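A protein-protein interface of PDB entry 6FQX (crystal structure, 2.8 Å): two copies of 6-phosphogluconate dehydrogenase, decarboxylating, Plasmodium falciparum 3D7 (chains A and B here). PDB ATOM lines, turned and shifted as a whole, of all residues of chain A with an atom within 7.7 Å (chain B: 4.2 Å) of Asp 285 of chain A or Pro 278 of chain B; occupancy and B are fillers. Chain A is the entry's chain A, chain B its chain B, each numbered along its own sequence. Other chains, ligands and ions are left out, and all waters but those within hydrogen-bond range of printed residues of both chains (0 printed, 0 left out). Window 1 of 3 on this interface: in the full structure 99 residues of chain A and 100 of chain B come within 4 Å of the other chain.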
ATOM      1  N   GLN A 194      -0.438  12.433   0.377  1.00  0.00           N
ATOM      2  CA  GLN A 194      -0.302  13.437   1.423  1.00  0.00           C
ATOM      3  C   GLN A 194       1.159  13.799   1.635  1.00  0.00           C
ATOM      4  O   GLN A 194       1.492  14.982   1.762  1.00  0.00           O
ATOM      5  CB  GLN A 194      -0.973  12.941   2.717  1.00  0.00           C
ATOM      6  CG  GLN A 194      -0.886  13.877   3.927  1.00  0.00           C
ATOM      7  CD  GLN A 194      -1.511  15.252   3.679  1.00  0.00           C
ATOM      8  OE1 GLN A 194      -2.329  15.433   2.778  1.00  0.00           O
ATOM      9  NE2 GLN A 194      -1.114  16.232   4.492  1.00  0.00           N
ATOM     10  N   ALA A 257     -11.539  17.924  -0.656  1.00  0.00           N
ATOM     11  CA  ALA A 257     -11.360  16.557  -1.153  1.00  0.00           C
ATOM     12  C   ALA A 257     -11.558  15.628   0.036  1.00  0.00           C
ATOM     13  O   ALA A 257     -10.615  15.366   0.789  1.00  0.00           O
ATOM     14  CB  ALA A 257      -9.985  16.379  -1.787  1.00  0.00           C
ATOM     15  N   ALA A 259     -12.587  12.169   2.333  1.00  0.00           N
ATOM     16  CA  ALA A 259     -12.210  10.756   2.402  1.00  0.00           C
ATOM     17  C   ALA A 259     -13.354   9.882   1.893  1.00  0.00           C
ATOM     18  O   ALA A 259     -14.353   9.677   2.594  1.00  0.00           O
ATOM     19  CB  ALA A 259     -11.831  10.390   3.834  1.00  0.00           C
ATOM     20  N   PRO A 278      -0.200   5.605  11.739  1.00  0.00           N
ATOM     21  CA  PRO A 278      -0.225   7.069  11.938  1.00  0.00           C
ATOM     22  C   PRO A 278      -0.196   7.886  10.661  1.00  0.00           C
ATOM     23  O   PRO A 278      -0.781   8.977  10.625  1.00  0.00           O
ATOM     24  CB  PRO A 278       1.055   7.326  12.745  1.00  0.00           C
ATOM     25  CG  PRO A 278       1.464   6.016  13.269  1.00  0.00           C
ATOM     26  CD  PRO A 278       1.039   5.015  12.263  1.00  0.00           C
ATOM     27  N   THR A 279       0.518   7.421   9.631  1.00  0.00           N
ATOM     28  CA  THR A 279       0.604   8.168   8.381  1.00  0.00           C
ATOM     29  C   THR A 279      -0.736   8.229   7.659  1.00  0.00           C
ATOM     30  O   THR A 279      -1.021   9.201   6.944  1.00  0.00           O
ATOM     31  CB  THR A 279       1.671   7.551   7.496  1.00  0.00           C
ATOM     32  OG1 THR A 279       2.864   7.394   8.272  1.00  0.00           O
ATOM     33  CG2 THR A 279       1.966   8.460   6.286  1.00  0.00           C
ATOM     34  N   MET A 280      -1.587   7.236   7.867  1.00  0.00           N
ATOM     35  CA  MET A 280      -2.901   7.299   7.260  1.00  0.00           C
ATOM     36  C   MET A 280      -3.881   8.120   8.087  1.00  0.00           C
ATOM     37  O   MET A 280      -4.811   8.712   7.527  1.00  0.00           O
ATOM     38  CB  MET A 280      -3.416   5.887   7.065  1.00  0.00           C
ATOM     39  CG  MET A 280      -4.764   5.844   6.424  1.00  0.00           C
ATOM     40  SD  MET A 280      -4.776   4.454   5.324  1.00  0.00           S
ATOM     41  CE  MET A 280      -3.775   3.266   6.231  1.00  0.00           C
ATOM     42  N   CYS A 281      -3.679   8.197   9.405  1.00  0.00           N
ATOM     43  CA  CYS A 281      -4.390   9.196  10.199  1.00  0.00           C
ATOM     44  C   CYS A 281      -4.173  10.582   9.621  1.00  0.00           C
ATOM     45  O   CYS A 281      -5.131  11.306   9.320  1.00  0.00           O
ATOM     46  CB  CYS A 281      -3.907   9.171  11.647  1.00  0.00           C
ATOM     47  SG  CYS A 281      -4.675   7.952  12.699  1.00  0.00           S
ATOM     48  N   ALA A 282      -2.899  10.942   9.422  1.00  0.00           N
ATOM     49  CA  ALA A 282      -2.544  12.275   8.954  1.00  0.00           C
ATOM     50  C   ALA A 282      -3.124  12.544   7.574  1.00  0.00           C
ATOM     51  O   ALA A 282      -3.588  13.657   7.293  1.00  0.00           O
ATOM     52  CB  ALA A 282      -1.023  12.437   8.955  1.00  0.00           C
ATOM     53  N   ALA A 283      -3.058  11.550   6.681  1.00  0.00           N
ATOM     54  CA  ALA A 283      -3.660  11.703   5.361  1.00  0.00           C
ATOM     55  C   ALA A 283      -5.170  11.885   5.457  1.00  0.00           C
ATOM     56  O   ALA A 283      -5.740  12.748   4.786  1.00  0.00           O
ATOM     57  CB  ALA A 283      -3.316  10.504   4.485  1.00  0.00           C
ATOM     58  N   LEU A 284      -5.838  11.097   6.297  1.00  0.00           N
ATOM     59  CA  LEU A 284      -7.288  11.234   6.425  1.00  0.00           C
ATOM     60  C   LEU A 284      -7.668  12.508   7.164  1.00  0.00           C
ATOM     61  O   LEU A 284      -8.700  13.112   6.855  1.00  0.00           O
ATOM     62  CB  LEU A 284      -7.881  10.027   7.143  1.00  0.00           C
ATOM     63  CG  LEU A 284      -7.898   8.724   6.356  1.00  0.00           C
ATOM     64  CD1 LEU A 284      -8.500   7.629   7.208  1.00  0.00           C
ATOM     65  CD2 LEU A 284      -8.673   8.909   5.081  1.00  0.00           C
ATOM     66  N   ASP A 285      -6.844  12.923   8.135  1.00  0.00           N
ATOM     67  CA  ASP A 285      -7.067  14.184   8.833  1.00  0.00           C
ATOM     68  C   ASP A 285      -7.084  15.325   7.843  1.00  0.00           C
ATOM     69  O   ASP A 285      -7.976  16.188   7.868  1.00  0.00           O
ATOM     70  CB  ASP A 285      -5.933  14.421   9.838  1.00  0.00           C
ATOM     71  CG  ASP A 285      -6.088  13.618  11.092  1.00  0.00           C
ATOM     72  OD1 ASP A 285      -7.254  13.489  11.540  1.00  0.00           O
ATOM     73  OD2 ASP A 285      -5.061  13.108  11.622  1.00  0.00           O
ATOM     74  N   ALA A 286      -6.091  15.317   6.947  1.00  0.00           N
ATOM     75  CA  ALA A 286      -5.945  16.344   5.931  1.00  0.00           C
ATOM     76  C   ALA A 286      -7.137  16.365   4.991  1.00  0.00           C
ATOM     77  O   ALA A 286      -7.656  17.439   4.667  1.00  0.00           O
ATOM     78  CB  ALA A 286      -4.642  16.112   5.170  1.00  0.00           C
ATOM     79  N   ARG A 287      -7.616  15.194   4.572  1.00  0.00           N
ATOM     80  CA  ARG A 287      -8.770  15.188   3.684  1.00  0.00           C
ATOM     81  C   ARG A 287     -10.038  15.610   4.413  1.00  0.00           C
ATOM     82  O   ARG A 287     -10.791  16.455   3.921  1.00  0.00           O
ATOM     83  CB  ARG A 287      -8.963  13.814   3.048  1.00  0.00           C
ATOM     84  CG  ARG A 287      -7.937  13.504   2.012  1.00  0.00           C
ATOM     85  CD  ARG A 287      -8.423  12.385   1.170  1.00  0.00           C
ATOM     86  NE  ARG A 287      -7.426  11.877   0.238  1.00  0.00           N
ATOM     87  CZ  ARG A 287      -7.740  11.326  -0.932  1.00  0.00           C
ATOM     88  NH1 ARG A 287      -9.019  11.240  -1.309  1.00  0.00           N
ATOM     89  NH2 ARG A 287      -6.782  10.869  -1.730  1.00  0.00           N
ATOM     90  N   ASN A 288     -10.268  15.077   5.607  1.00  0.00           N
ATOM     91  CA  ASN A 288     -11.491  15.431   6.310  1.00  0.00           C
ATOM     92  C   ASN A 288     -11.489  16.887   6.751  1.00  0.00           C
ATOM     93  O   ASN A 288     -12.543  17.530   6.736  1.00  0.00           O
ATOM     94  CB  ASN A 288     -11.699  14.506   7.503  1.00  0.00           C
ATOM     95  CG  ASN A 288     -11.965  13.076   7.074  1.00  0.00           C
ATOM     96  OD1 ASN A 288     -12.557  12.828   6.014  1.00  0.00           O
ATOM     97  ND2 ASN A 288     -11.521  12.125   7.890  1.00  0.00           N
ATOM     98  N   ILE A 289     -10.326  17.451   7.070  1.00  0.00           N
ATOM     99  CA  ILE A 289     -10.309  18.854   7.465  1.00  0.00           C
ATOM    100  C   ILE A 289     -10.667  19.748   6.277  1.00  0.00           C
ATOM    101  O   ILE A 289     -11.235  20.825   6.455  1.00  0.00           O
ATOM    102  CB  ILE A 289      -8.934  19.212   8.058  1.00  0.00           C
ATOM    103  CG1 ILE A 289      -8.924  18.907   9.542  1.00  0.00           C
ATOM    104  CG2 ILE A 289      -8.633  20.690   7.951  1.00  0.00           C
ATOM    105  CD1 ILE A 289      -9.933  19.718  10.325  1.00  0.00           C
ATOM    106  N   SER A 290     -10.349  19.328   5.050  1.00  0.00           N
ATOM    107  CA  SER A 290     -10.576  20.196   3.896  1.00  0.00           C
ATOM    108  C   SER A 290     -12.059  20.420   3.592  1.00  0.00           C
ATOM    109  O   SER A 290     -12.411  21.478   3.066  1.00  0.00           O
ATOM    110  CB  SER A 290      -9.836  19.651   2.669  1.00  0.00           C
ATOM    111  OG  SER A 290     -10.358  18.426   2.209  1.00  0.00           O
ATOM    112  N   VAL A 291     -12.945  19.491   3.966  1.00  0.00           N
ATOM    113  CA  VAL A 291     -14.385  19.670   3.737  1.00  0.00           C
ATOM    114  C   VAL A 291     -14.931  20.880   4.475  1.00  0.00           C
ATOM    115  O   VAL A 291     -15.840  21.551   3.975  1.00  0.00           O
ATOM    116  CB  VAL A 291     -15.172  18.383   4.083  1.00  0.00           C
ATOM    117  CG1 VAL A 291     -16.574  18.430   3.519  1.00  0.00           C
ATOM    118  CG2 VAL A 291     -14.467  17.191   3.374  1.00  0.00           C
ATOM    119  N   PHE A 292     -14.400  21.201   5.647  1.00  0.00           N
ATOM    120  CA  PHE A 292     -14.982  22.320   6.370  1.00  0.00           C
ATOM    121  C   PHE A 292     -14.297  23.620   5.960  1.00  0.00           C
ATOM    122  O   PHE A 292     -13.669  24.307   6.765  1.00  0.00           O
ATOM    123  CB  PHE A 292     -14.902  22.071   7.865  1.00  0.00           C
ATOM    124  CG  PHE A 292     -15.512  20.769   8.281  1.00  0.00           C
ATOM    125  CD1 PHE A 292     -16.888  20.658   8.451  1.00  0.00           C
ATOM    126  CD2 PHE A 292     -14.713  19.651   8.498  1.00  0.00           C
ATOM    127  CE1 PHE A 292     -17.455  19.443   8.828  1.00  0.00           C
ATOM    128  CE2 PHE A 292     -15.271  18.434   8.881  1.00  0.00           C
ATOM    129  CZ  PHE A 292     -16.647  18.329   9.047  1.00  0.00           C
ATOM    130  N   PRO A 421       1.392  17.023   8.887  1.00  0.00           N
ATOM    131  CA  PRO A 421       1.033  15.901   9.761  1.00  0.00           C
ATOM    132  C   PRO A 421       1.637  14.562   9.364  1.00  0.00           C
ATOM    133  O   PRO A 421       2.105  13.830  10.249  1.00  0.00           O
ATOM    134  CB  PRO A 421      -0.496  15.881   9.656  1.00  0.00           C
ATOM    135  CG  PRO A 421      -0.828  16.641   8.420  1.00  0.00           C
ATOM    136  CD  PRO A 421       0.202  17.702   8.345  1.00  0.00           C
ATOM    137  N   ALA A 425       3.877  12.405  11.799  1.00  0.00           N
ATOM    138  CA  ALA A 425       3.407  11.103  12.239  1.00  0.00           C
ATOM    139  C   ALA A 425       4.426  10.011  11.917  1.00  0.00           C
ATOM    140  O   ALA A 425       4.678   9.121  12.737  1.00  0.00           O
ATOM    141  CB  ALA A 425       2.052  10.818  11.593  1.00  0.00           C
ATOM    142  N   PRO B 276     -11.996  14.957  12.049  1.00  0.00           N
ATOM    143  CA  PRO B 276     -10.604  14.618  12.408  1.00  0.00           C
ATOM    144  C   PRO B 276     -10.329  14.791  13.900  1.00  0.00           C
ATOM    145  O   PRO B 276     -10.618  15.832  14.496  1.00  0.00           O
ATOM    146  CB  PRO B 276      -9.774  15.590  11.566  1.00  0.00           C
ATOM    147  CG  PRO B 276     -10.686  16.754  11.371  1.00  0.00           C
ATOM    148  CD  PRO B 276     -12.085  16.201  11.266  1.00  0.00           C
ATOM    149  N   CYS B 277      -9.693  13.781  14.474  1.00  0.00           N
ATOM    150  CA  CYS B 277      -9.274  13.782  15.873  1.00  0.00           C
ATOM    151  C   CYS B 277      -7.840  13.276  15.902  1.00  0.00           C
ATOM    152  O   CYS B 277      -7.576  12.135  16.298  1.00  0.00           O
ATOM    153  CB  CYS B 277     -10.186  12.895  16.728  1.00  0.00           C
ATOM    154  SG  CYS B 277     -11.933  13.424  16.970  1.00  0.00           S
ATOM    155  N   PRO B 278      -6.885  14.086  15.414  1.00  0.00           N
ATOM    156  CA  PRO B 278      -5.498  13.597  15.303  1.00  0.00           C
ATOM    157  C   PRO B 278      -4.847  13.290  16.648  1.00  0.00           C
ATOM    158  O   PRO B 278      -4.016  12.372  16.742  1.00  0.00           O
ATOM    159  CB  PRO B 278      -4.781  14.754  14.594  1.00  0.00           C
ATOM    160  CG  PRO B 278      -5.873  15.629  14.027  1.00  0.00           C
ATOM    161  CD  PRO B 278      -7.007  15.489  14.977  1.00  0.00           C
ATOM    162  N   THR B 279      -5.163  14.079  17.684  1.00  0.00           N
ATOM    163  CA  THR B 279      -4.620  13.829  19.017  1.00  0.00           C
ATOM    164  C   THR B 279      -5.106  12.498  19.573  1.00  0.00           C
ATOM    165  O   THR B 279      -4.453  11.911  20.438  1.00  0.00           O
ATOM    166  CB  THR B 279      -5.027  14.944  19.987  1.00  0.00           C
ATOM    167  OG1 THR B 279      -4.757  16.238  19.435  1.00  0.00           O
ATOM    168  CG2 THR B 279      -4.318  14.825  21.330  1.00  0.00           C
ATOM    169  N   MET B 280      -6.259  12.018  19.127  1.00  0.00           N
ATOM    170  CA  MET B 280      -6.751  10.740  19.617  1.00  0.00           C
ATOM    171  C   MET B 280      -6.148   9.559  18.831  1.00  0.00           C
ATOM    172  O   MET B 280      -6.031   8.456  19.377  1.00  0.00           O
ATOM    173  CB  MET B 280      -8.296  10.834  19.576  1.00  0.00           C
ATOM    174  CG  MET B 280      -9.195   9.810  20.365  1.00  0.00           C
ATOM    175  SD  MET B 280     -10.890  10.482  20.855  1.00  0.00           S
ATOM    176  CE  MET B 280     -10.842  12.310  21.079  1.00  0.00           C
ATOM    177  N   CYS B 281      -5.724   9.771  17.581  1.00  0.00           N
ATOM    178  CA  CYS B 281      -4.862   8.799  16.917  1.00  0.00           C
ATOM    179  C   CYS B 281      -3.598   8.575  17.728  1.00  0.00           C
ATOM    180  O   CYS B 281      -3.223   7.435  18.028  1.00  0.00           O
ATOM    181  CB  CYS B 281      -4.470   9.270  15.521  1.00  0.00           C
ATOM    182  SG  CYS B 281      -5.627   9.024  14.156  1.00  0.00           S
ATOM    183  N   ALA B 282      -2.932   9.669  18.097  1.00  0.00           N
ATOM    184  CA  ALA B 282      -1.643   9.568  18.762  1.00  0.00           C
ATOM    185  C   ALA B 282      -1.765   8.802  20.069  1.00  0.00           C
ATOM    186  O   ALA B 282      -0.930   7.939  20.374  1.00  0.00           O
ATOM    187  CB  ALA B 282      -1.077  10.966  18.991  1.00  0.00           C
ATOM    188  N   GLN B 337     -10.984  19.480  19.337  1.00  0.00           N
ATOM    189  CA  GLN B 337     -11.377  18.334  18.517  1.00  0.00           C
ATOM    190  C   GLN B 337     -12.522  17.566  19.172  1.00  0.00           C
ATOM    191  O   GLN B 337     -13.513  17.236  18.515  1.00  0.00           O
ATOM    192  CB  GLN B 337     -10.211  17.371  18.287  1.00  0.00           C
ATOM    193  CG  GLN B 337      -8.868  17.958  17.946  1.00  0.00           C
ATOM    194  CD  GLN B 337      -7.769  16.897  17.995  1.00  0.00           C
ATOM    195  OE1 GLN B 337      -8.024  15.715  18.281  1.00  0.00           O
ATOM    196  NE2 GLN B 337      -6.551  17.306  17.705  1.00  0.00           N
ATOM    197  N   ALA B 425       0.700  16.075  16.707  1.00  0.00           N
ATOM    198  CA  ALA B 425      -0.599  16.039  16.054  1.00  0.00           C
ATOM    199  C   ALA B 425      -1.399  17.271  16.424  1.00  0.00           C
ATOM    200  O   ALA B 425      -2.032  17.902  15.563  1.00  0.00           O
ATOM    201  CB  ALA B 425      -1.338  14.762  16.435  1.00  0.00           C
ATOM    202  N   TYR B 429      -2.688  19.774  13.690  1.00  0.00           N
ATOM    203  CA  TYR B 429      -4.129  19.982  13.594  1.00  0.00           C
ATOM    204  C   TYR B 429      -4.459  21.469  13.626  1.00  0.00           C
ATOM    205  O   TYR B 429      -5.290  21.961  12.846  1.00  0.00           O
ATOM    206  CB  TYR B 429      -4.850  19.228  14.710  1.00  0.00           C
ATOM    207  CG  TYR B 429      -6.307  19.597  14.839  1.00  0.00           C
ATOM    208  CD1 TYR B 429      -7.275  19.036  14.010  1.00  0.00           C
ATOM    209  CD2 TYR B 429      -6.715  20.522  15.797  1.00  0.00           C
ATOM    210  CE1 TYR B 429      -8.607  19.395  14.126  1.00  0.00           C
ATOM    211  CE2 TYR B 429      -8.034  20.889  15.916  1.00  0.00           C
ATOM    212  CZ  TYR B 429      -8.976  20.325  15.083  1.00  0.00           C
ATOM    213  OH  TYR B 429     -10.280  20.712  15.238  1.00  0.00           O
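SG of Cys 281 of chain A is disulfide-bonded to SG of Cys 281 of chain B.
Among the printed residues, pairs that only touch across the chains: Ile 289 of chain A with Pro 276 of chain B (3.2 Å), Asp 285 of chain A with Pro 276 of chain B (3.3 Å), Asp 285 of chain A with Pro 278 of chain B (3.4 Å) and Asp 285 of chain A with Cys 277 of chain B (3.8 Å).
Of the 10 printed residues of chain B, 4 touch a printed residue of chain A. Printed residues of chain B that touch a printed residue of chain A: Pro 276, Cys 277, Pro 278 and Cys 281. Hydrophobic or aromatic side chains of chain B within 4 Å of the printed part of chain A: Pro 276 and Pro 278. Hydrophobic or aromatic side chains of chain A that line the printed part of chain B: Ile 289. Among the printed residues, 5 pairs touch across the chains.
Cys 281 of chain B touches its own counterpart, Cys 281 of chain A. Positions printed for both chains: 278, 279, 280, 281, 282 and 425. Of the 5 pairs that touch across the chains among the printed residues, 1 has its exchanged pair printed and touching as well.
Pro 278 of chain B touches just one residue of chain A: Asp 285. Of the printed residues of chain A, Cys 277 of chain B touches Asp 285. Of the printed residues of chain B, Ile 289 of chain A touches Pro 276 (3.2 Å). The nearest printed residue of chain B that does not touch Asp 285 of chain A is Cys 281 of chain B (4.8 Å). The nearest residue of chain A that does not touch Pro 278 of chain B is Cys 281 of chain A (6.0 Å). The nearest printed residue of chain A that does not touch Cys 281 of chain B is Asp 285 of chain A (4.8 Å).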
